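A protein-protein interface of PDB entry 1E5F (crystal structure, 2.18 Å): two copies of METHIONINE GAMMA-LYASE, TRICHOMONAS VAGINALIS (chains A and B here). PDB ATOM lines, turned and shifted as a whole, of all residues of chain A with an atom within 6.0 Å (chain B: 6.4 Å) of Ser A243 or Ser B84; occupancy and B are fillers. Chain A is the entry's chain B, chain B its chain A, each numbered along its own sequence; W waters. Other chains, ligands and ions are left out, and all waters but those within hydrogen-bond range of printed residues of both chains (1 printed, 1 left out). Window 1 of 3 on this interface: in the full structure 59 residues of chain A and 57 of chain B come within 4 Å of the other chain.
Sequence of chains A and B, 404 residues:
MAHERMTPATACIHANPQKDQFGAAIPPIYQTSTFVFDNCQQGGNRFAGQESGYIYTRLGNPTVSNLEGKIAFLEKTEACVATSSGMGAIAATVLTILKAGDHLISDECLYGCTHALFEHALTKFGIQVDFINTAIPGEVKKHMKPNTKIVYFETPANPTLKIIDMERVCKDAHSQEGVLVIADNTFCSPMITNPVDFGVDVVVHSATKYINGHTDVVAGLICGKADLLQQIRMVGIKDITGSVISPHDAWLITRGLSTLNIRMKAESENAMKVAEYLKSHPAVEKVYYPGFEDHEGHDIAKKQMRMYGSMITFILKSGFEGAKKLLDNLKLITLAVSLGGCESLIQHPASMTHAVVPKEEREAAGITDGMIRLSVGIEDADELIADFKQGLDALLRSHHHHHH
Ser A243 touches just these residues of chain B: Ser B84 (3.8 Å), Thr B241 (3.6 Å) and Gly B242 (3.0 Å). Of chain A, only Ser A84, Gly A242, Ser A243 and Val A244 come within 4 Å of Ser B84. Of the printed residues of chain A, Gly B88 touches Thr A241 and Gly A242. Of the printed residues of chain A, Gly B242 touches Ser A84, Ser A85, Gly A88 and Ser A243. Printed residues of chain B within 4 Å of Thr A241: Gly B88 (3.4 Å), Thr B241 (3.3 Å) and Ser B243 (3.5 Å). Of the printed residues of chain B, Gly A242 touches Ser B84, Ser B85, Gly B88 and Ser B243. The nearest printed residue of chain A that does not touch Ser B85 is Ser A243 (4.6 Å).
Of the 17 printed residues of chain B, 7 touch a printed residue of chain A. Hydrophobic or aromatic side chains of chain B that line the printed part of chain A: Val B244. Of the 14 printed residues of chain A, 7 touch a printed residue of chain B. Among the printed residues, no Asp or Glu carboxylate lies within 4 Å of a Lys or Arg side-chain nitrogen of the other chain.
The backbone NH of Val A244 lies within hydrogen-bond range of the side-chain hydroxyl of Ser B84 (3.3 Å). The backbone carbonyl oxygen (O) of Gly A242 is in hydrogen-bond range of the side-chain hydroxyl (OG) of Ser B243, 2.8 Å away. The backbone NH (N) of Val B244 sits at hydrogen-bond distance from the side-chain hydroxyl (OG) of Ser A84, at 3.2 Å. OG of Ser B84 sits at hydrogen-bond distance from OG of Ser A84, at 3.0 Å. The backbone carbonyl oxygen (O) of Gly A242 sits at hydrogen-bond distance from the side-chain hydroxyl (OG) of Ser B85 (2.8 Å). OG of Ser A85 sits at hydrogen-bond distance from O of Gly B242 (2.8 Å). The side-chain hydroxyl (OG) of Ser B84 lies within hydrogen-bond range of the backbone carbonyl oxygen (O) of Gly A242 (3.2 Å). O of Gly B242 sits at hydrogen-bond distance from OG of Ser A243 (3.0 Å). The backbone carbonyl oxygen of Gly B242 lies within hydrogen-bond range of the side-chain hydroxyl of Ser A84, at 3.1 Å.
Water W1 lies within hydrogen-bond range of the backbone carbonyl oxygen of Val B244 and the backbone carbonyl oxygen of Ser A84.
O of Ser B85 is in hydrogen-bond range of OG1 of Thr B83 (2.6 Å). O of Ser A85 is in hydrogen-bond range of OG1 of Thr A83, 2.8 Å away. The backbone NH (N) of Gly A242 sits at hydrogen-bond distance from the backbone carbonyl oxygen (O) of Ile A237. N of Ser B243 sits close to OG1 of Thr B241, 3.1 Å away. The side-chain hydroxyl (OG) of Ser B243 sits at hydrogen-bond distance from the side-chain hydroxyl (OG) of Ser B84 (3.1 Å). OG of Ser B85 is in hydrogen-bond range of N of Gly B88 (3.0 Å).
Ser B84 touches its own counterpart, Ser A84. Gly A88 touches Thr B241, and with the chains exchanged Thr A241 touches Gly B88. Thr B241 touches its own counterpart, Thr A241. Gly A242 touches Ser B243, and with the chains exchanged Ser A243 touches Gly B242. 11 positions are printed for both chains. Of the 19 pairs that touch across the chains among the printed residues, 18 have their exchanged pair printed and touching as well.
Among the printed residues, merely in contact across the chains: Thr A241 with Thr B241 (3.3 Å), Gly A88 with Thr B241 (3.4 Å), Thr A241 with Gly B88 (3.4 Å), Thr A241 with Ser B243 (3.5 Å), Ser A243 with Thr B241 (3.6 Å), Gly A88 with Gly B242 (3.7 Å), Gly A242 with Gly B88 (3.7 Å), Ser A84 with Ser B243 (3.7 Å), Ser A243 with Ser B84 (3.8 Å) and Val A244 with Ser B85 (3.999 Å).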
ATOM      1  N   ALA A  82       5.572  16.713  -6.778  1.00  0.00           N
ATOM      2  CA  ALA A  82       4.693  16.867  -7.955  1.00  0.00           C
ATOM      3  C   ALA A  82       3.293  17.215  -7.515  1.00  0.00           C
ATOM      4  O   ALA A  82       2.986  16.920  -6.325  1.00  0.00           O
ATOM      5  CB  ALA A  82       4.577  15.538  -8.762  1.00  0.00           C
ATOM      6  N   THR A  83       2.508  17.959  -8.305  1.00  0.00           N
ATOM      7  CA  THR A  83       1.215  18.398  -7.803  1.00  0.00           C
ATOM      8  C   THR A  83       0.229  18.253  -8.956  1.00  0.00           C
ATOM      9  O   THR A  83       0.707  18.038 -10.075  1.00  0.00           O
ATOM     10  CB  THR A  83       1.155  19.926  -7.484  1.00  0.00           C
ATOM     11  OG1 THR A  83       1.424  20.604  -8.700  1.00  0.00           O
ATOM     12  CG2 THR A  83       2.066  20.234  -6.292  1.00  0.00           C
ATOM     13  N   SER A  84      -1.066  18.455  -8.792  1.00  0.00           N
ATOM     14  CA  SER A  84      -2.026  18.225  -9.837  1.00  0.00           C
ATOM     15  C   SER A  84      -2.240  19.477 -10.684  1.00  0.00           C
ATOM     16  O   SER A  84      -2.995  19.334 -11.630  1.00  0.00           O
ATOM     17  CB  SER A  84      -3.360  17.793  -9.310  1.00  0.00           C
ATOM     18  OG  SER A  84      -3.983  18.722  -8.497  1.00  0.00           O
ATOM     19  N   SER A  85      -1.465  20.513 -10.600  1.00  0.00           N
ATOM     20  CA  SER A  85      -1.446  21.561 -11.684  1.00  0.00           C
ATOM     21  C   SER A  85      -0.306  22.516 -11.331  1.00  0.00           C
ATOM     22  O   SER A  85       0.087  22.610 -10.203  1.00  0.00           O
ATOM     23  CB  SER A  85      -2.658  22.483 -11.736  1.00  0.00           C
ATOM     24  OG  SER A  85      -2.830  23.061 -10.449  1.00  0.00           O
ATOM     25  N   GLY A  88      -1.192  24.706  -8.640  1.00  0.00           N
ATOM     26  CA  GLY A  88      -1.052  23.992  -7.308  1.00  0.00           C
ATOM     27  C   GLY A  88       0.392  23.983  -6.913  1.00  0.00           C
ATOM     28  O   GLY A  88       0.716  23.991  -5.697  1.00  0.00           O
ATOM     29  N   ALA A  89       1.306  23.913  -7.842  1.00  0.00           N
ATOM     30  CA  ALA A  89       2.725  23.948  -7.382  1.00  0.00           C
ATOM     31  C   ALA A  89       3.096  25.303  -6.882  1.00  0.00           C
ATOM     32  O   ALA A  89       3.788  25.410  -5.849  1.00  0.00           O
ATOM     33  CB  ALA A  89       3.607  23.559  -8.603  1.00  0.00           C
ATOM     34  N   ALA A  92       1.098  25.760  -3.470  1.00  0.00           N
ATOM     35  CA  ALA A  92       1.594  24.987  -2.334  1.00  0.00           C
ATOM     36  C   ALA A  92       2.936  25.516  -1.794  1.00  0.00           C
ATOM     37  O   ALA A  92       3.124  25.592  -0.560  1.00  0.00           O
ATOM     38  CB  ALA A  92       1.643  23.485  -2.647  1.00  0.00           C
ATOM     39  N   GLY A 236       1.689  22.560   2.602  1.00  0.00           N
ATOM     40  CA  GLY A 236       1.039  23.022   1.402  1.00  0.00           C
ATOM     41  C   GLY A 236       0.304  21.988   0.544  1.00  0.00           C
ATOM     42  O   GLY A 236      -0.782  22.323   0.047  1.00  0.00           O
ATOM     43  N   ILE A 237       0.811  20.770   0.434  1.00  0.00           N
ATOM     44  CA  ILE A 237       0.070  19.725  -0.257  1.00  0.00           C
ATOM     45  C   ILE A 237      -0.911  19.053   0.710  1.00  0.00           C
ATOM     46  O   ILE A 237      -2.086  18.862   0.382  1.00  0.00           O
ATOM     47  CB  ILE A 237       0.935  18.645  -0.901  1.00  0.00           C
ATOM     48  CG1 ILE A 237       2.035  19.169  -1.841  1.00  0.00           C
ATOM     49  CG2 ILE A 237       0.188  17.527  -1.652  1.00  0.00           C
ATOM     50  CD1 ILE A 237       1.575  20.015  -2.960  1.00  0.00           C
ATOM     51  N   THR A 241      -3.491  22.963  -0.131  1.00  0.00           N
ATOM     52  CA  THR A 241      -4.050  22.962  -1.473  1.00  0.00           C
ATOM     53  C   THR A 241      -4.706  21.616  -1.710  1.00  0.00           C
ATOM     54  O   THR A 241      -5.555  21.548  -2.601  1.00  0.00           O
ATOM     55  CB  THR A 241      -2.922  23.173  -2.451  1.00  0.00           C
ATOM     56  OG1 THR A 241      -2.033  22.064  -2.358  1.00  0.00           O
ATOM     57  CG2 THR A 241      -2.138  24.414  -2.019  1.00  0.00           C
ATOM     58  N   GLY A 242      -4.155  20.514  -1.174  1.00  0.00           N
ATOM     59  CA  GLY A 242      -4.792  19.228  -1.504  1.00  0.00           C
ATOM     60  C   GLY A 242      -4.515  18.955  -3.026  1.00  0.00           C
ATOM     61  O   GLY A 242      -5.298  18.301  -3.713  1.00  0.00           O
ATOM     62  N   SER A 243      -3.447  19.493  -3.559  1.00  0.00           N
ATOM     63  CA  SER A 243      -3.191  19.301  -4.967  1.00  0.00           C
ATOM     64  C   SER A 243      -2.377  18.038  -5.210  1.00  0.00           C
ATOM     65  O   SER A 243      -1.242  18.120  -5.628  1.00  0.00           O
ATOM     66  CB  SER A 243      -2.420  20.548  -5.498  1.00  0.00           C
ATOM     67  OG  SER A 243      -2.260  20.414  -6.920  1.00  0.00           O
ATOM     68  N   VAL A 244      -3.016  16.905  -5.155  1.00  0.00           N
ATOM     69  CA  VAL A 244      -2.501  15.589  -5.289  1.00  0.00           C
ATOM     70  C   VAL A 244      -2.515  15.015  -6.671  1.00  0.00           C
ATOM     71  O   VAL A 244      -3.644  14.809  -7.264  1.00  0.00           O
ATOM     72  CB  VAL A 244      -3.262  14.641  -4.310  1.00  0.00           C
ATOM     73  CG1 VAL A 244      -2.718  13.238  -4.377  1.00  0.00           C
ATOM     74  CG2 VAL A 244      -3.126  15.240  -2.908  1.00  0.00           C
ATOM     75  N   ILE A 245      -1.338  14.906  -7.238  1.00  0.00           N
ATOM     76  CA  ILE A 245      -1.341  14.361  -8.636  1.00  0.00           C
ATOM     77  C   ILE A 245      -1.819  12.928  -8.672  1.00  0.00           C
ATOM     78  O   ILE A 245      -1.553  12.091  -7.858  1.00  0.00           O
ATOM     79  CB  ILE A 245       0.069  14.502  -9.247  1.00  0.00           C
ATOM     80  CG1 ILE A 245      -0.002  14.212 -10.777  1.00  0.00           C
ATOM     81  CG2 ILE A 245       1.055  13.627  -8.539  1.00  0.00           C
ATOM     82  CD1 ILE A 245       1.395  14.705 -11.362  1.00  0.00           C
ATOM     83  N   ALA B  82     -15.475  18.988  -8.570  1.00  0.00           N
ATOM     84  CA  ALA B  82     -14.620  17.867  -8.178  1.00  0.00           C
ATOM     85  C   ALA B  82     -13.203  18.288  -8.028  1.00  0.00           C
ATOM     86  O   ALA B  82     -12.825  19.312  -8.588  1.00  0.00           O
ATOM     87  CB  ALA B  82     -14.603  16.743  -9.222  1.00  0.00           C
ATOM     88  N   THR B  83     -12.444  17.656  -7.143  1.00  0.00           N
ATOM     89  CA  THR B  83     -11.133  18.089  -6.887  1.00  0.00           C
ATOM     90  C   THR B  83     -10.224  16.834  -6.786  1.00  0.00           C
ATOM     91  O   THR B  83     -10.728  15.724  -6.828  1.00  0.00           O
ATOM     92  CB  THR B  83     -10.946  18.878  -5.594  1.00  0.00           C
ATOM     93  OG1 THR B  83     -11.090  17.983  -4.473  1.00  0.00           O
ATOM     94  CG2 THR B  83     -11.829  20.110  -5.521  1.00  0.00           C
ATOM     95  N   SER B  84      -8.925  17.158  -6.660  1.00  0.00           N
ATOM     96  CA  SER B  84      -7.946  16.095  -6.647  1.00  0.00           C
ATOM     97  C   SER B  84      -7.621  15.622  -5.226  1.00  0.00           C
ATOM     98  O   SER B  84      -6.775  14.772  -5.174  1.00  0.00           O
ATOM     99  CB  SER B  84      -6.722  16.418  -7.523  1.00  0.00           C
ATOM    100  OG  SER B  84      -5.849  17.219  -6.727  1.00  0.00           O
ATOM    101  N   SER B  85      -8.413  15.892  -4.206  1.00  0.00           N
ATOM    102  CA  SER B  85      -8.320  15.238  -2.905  1.00  0.00           C
ATOM    103  C   SER B  85      -9.447  15.866  -2.050  1.00  0.00           C
ATOM    104  O   SER B  85      -9.919  16.960  -2.349  1.00  0.00           O
ATOM    105  CB  SER B  85      -7.043  15.367  -2.113  1.00  0.00           C
ATOM    106  OG  SER B  85      -6.781  16.786  -1.879  1.00  0.00           O
ATOM    107  N   GLY B  86      -9.853  15.078  -1.064  1.00  0.00           N
ATOM    108  CA  GLY B  86     -10.828  15.605  -0.097  1.00  0.00           C
ATOM    109  C   GLY B  86     -10.221  16.854   0.549  1.00  0.00           C
ATOM    110  O   GLY B  86     -11.003  17.792   0.697  1.00  0.00           O
ATOM    111  N   GLY B  88      -8.403  19.001  -0.750  1.00  0.00           N
ATOM    112  CA  GLY B  88      -8.534  20.082  -1.749  1.00  0.00           C
ATOM    113  C   GLY B  88      -9.959  20.595  -1.845  1.00  0.00           C
ATOM    114  O   GLY B  88     -10.167  21.772  -2.109  1.00  0.00           O
ATOM    115  N   ALA B  89     -10.954  19.711  -1.714  1.00  0.00           N
ATOM    116  CA  ALA B  89     -12.332  20.193  -1.698  1.00  0.00           C
ATOM    117  C   ALA B  89     -12.622  21.114  -0.476  1.00  0.00           C
ATOM    118  O   ALA B  89     -13.181  22.191  -0.625  1.00  0.00           O
ATOM    119  CB  ALA B  89     -13.239  19.025  -1.590  1.00  0.00           C
ATOM    120  N   THR B 208     -12.203   9.834  -2.343  1.00  0.00           N
ATOM    121  CA  THR B 208     -11.292   8.772  -2.230  1.00  0.00           C
ATOM    122  C   THR B 208     -11.908   7.625  -1.389  1.00  0.00           C
ATOM    123  O   THR B 208     -11.389   6.464  -1.372  1.00  0.00           O
ATOM    124  CB  THR B 208     -10.109   9.165  -1.331  1.00  0.00           C
ATOM    125  OG1 THR B 208      -9.759  10.459  -1.764  1.00  0.00           O
ATOM    126  CG2 THR B 208      -8.980   8.168  -1.221  1.00  0.00           C
ATOM    127  N   VAL B 218      -7.603   9.235  -5.403  1.00  0.00           N
ATOM    128  CA  VAL B 218      -7.676  10.215  -4.320  1.00  0.00           C
ATOM    129  C   VAL B 218      -8.382  11.408  -5.015  1.00  0.00           C
ATOM    130  O   VAL B 218      -7.830  11.909  -5.963  1.00  0.00           O
ATOM    131  CB  VAL B 218      -6.308  10.685  -3.732  1.00  0.00           C
ATOM    132  CG1 VAL B 218      -6.509  11.786  -2.705  1.00  0.00           C
ATOM    133  CG2 VAL B 218      -5.571   9.532  -3.069  1.00  0.00           C
ATOM    134  N   ALA B 219      -9.518  11.839  -4.504  1.00  0.00           N
ATOM    135  CA  ALA B 219     -10.222  12.941  -5.076  1.00  0.00           C
ATOM    136  C   ALA B 219     -11.227  13.478  -4.072  1.00  0.00           C
ATOM    137  O   ALA B 219     -11.672  12.834  -3.027  1.00  0.00           O
ATOM    138  CB  ALA B 219     -11.049  12.407  -6.267  1.00  0.00           C
ATOM    139  N   GLY B 220     -11.608  14.702  -4.364  1.00  0.00           N
ATOM    140  CA  GLY B 220     -12.608  15.380  -3.492  1.00  0.00           C
ATOM    141  C   GLY B 220     -13.821  15.860  -4.308  1.00  0.00           C
ATOM    142  O   GLY B 220     -13.716  15.989  -5.522  1.00  0.00           O
ATOM    143  N   THR B 241      -5.974  26.658  -4.873  1.00  0.00           N
ATOM    144  CA  THR B 241      -5.403  25.330  -4.512  1.00  0.00           C
ATOM    145  C   THR B 241      -4.759  24.718  -5.759  1.00  0.00           C
ATOM    146  O   THR B 241      -3.929  23.828  -5.571  1.00  0.00           O
ATOM    147  CB  THR B 241      -6.427  24.382  -3.973  1.00  0.00           C
ATOM    148  OG1 THR B 241      -7.358  24.155  -4.967  1.00  0.00           O
ATOM    149  CG2 THR B 241      -7.153  24.915  -2.736  1.00  0.00           C
ATOM    150  N   GLY B 242      -5.347  24.882  -6.943  1.00  0.00           N
ATOM    151  CA  GLY B 242      -4.790  24.149  -8.107  1.00  0.00           C
ATOM    152  C   GLY B 242      -5.047  22.677  -7.924  1.00  0.00           C
ATOM    153  O   GLY B 242      -4.355  21.820  -8.508  1.00  0.00           O
ATOM    154  N   SER B 243      -6.157  22.364  -7.244  1.00  0.00           N
ATOM    155  CA  SER B 243      -6.498  20.987  -6.961  1.00  0.00           C
ATOM    156  C   SER B 243      -7.326  20.448  -8.094  1.00  0.00           C
ATOM    157  O   SER B 243      -8.532  20.385  -8.043  1.00  0.00           O
ATOM    158  CB  SER B 243      -7.297  20.923  -5.602  1.00  0.00           C
ATOM    159  OG  SER B 243      -7.351  19.533  -5.208  1.00  0.00           O
ATOM    160  N   VAL B 244      -6.716  20.196  -9.241  1.00  0.00           N
ATOM    161  CA  VAL B 244      -7.414  19.857 -10.433  1.00  0.00           C
ATOM    162  C   VAL B 244      -7.460  18.305 -10.591  1.00  0.00           C
ATOM    163  O   VAL B 244      -6.406  17.696 -10.841  1.00  0.00           O
ATOM    164  CB  VAL B 244      -6.594  20.491 -11.584  1.00  0.00           C
ATOM    165  CG1 VAL B 244      -7.208  19.985 -12.881  1.00  0.00           C
ATOM    166  CG2 VAL B 244      -6.644  22.012 -11.544  1.00  0.00           C
ATOM    167  N   ILE B 245      -8.644  17.757 -10.626  1.00  0.00           N
ATOM    168  CA  ILE B 245      -8.766  16.282 -10.772  1.00  0.00           C
ATOM    169  C   ILE B 245      -8.295  15.867 -12.154  1.00  0.00           C
ATOM    170  O   ILE B 245      -8.609  16.477 -13.162  1.00  0.00           O
ATOM    171  CB  ILE B 245     -10.141  15.767 -10.410  1.00  0.00           C
ATOM    172  CG1 ILE B 245     -10.288  14.249 -10.289  1.00  0.00           C
ATOM    173  CG2 ILE B 245     -11.163  16.305 -11.404  1.00  0.00           C
ATOM    174  CD1 ILE B 245     -11.645  13.721  -9.709  1.00  0.00           C
ATOM    175  N   SER B 246      -7.678  14.764 -12.259  1.00  0.00           N
ATOM    176  CA  SER B 246      -7.337  14.060 -13.531  1.00  0.00           C
ATOM    177  C   SER B 246      -8.675  13.600 -14.127  1.00  0.00           C
ATOM    178  O   SER B 246      -9.350  12.827 -13.472  1.00  0.00           O
ATOM    179  CB  SER B 246      -6.595  12.762 -13.272  1.00  0.00           C
ATOM    180  OG  SER B 246      -6.395  11.988 -14.477  1.00  0.00           O
HETATM  181  O   HOH W   1      -4.745  17.169 -13.061  1.00  0.00           O
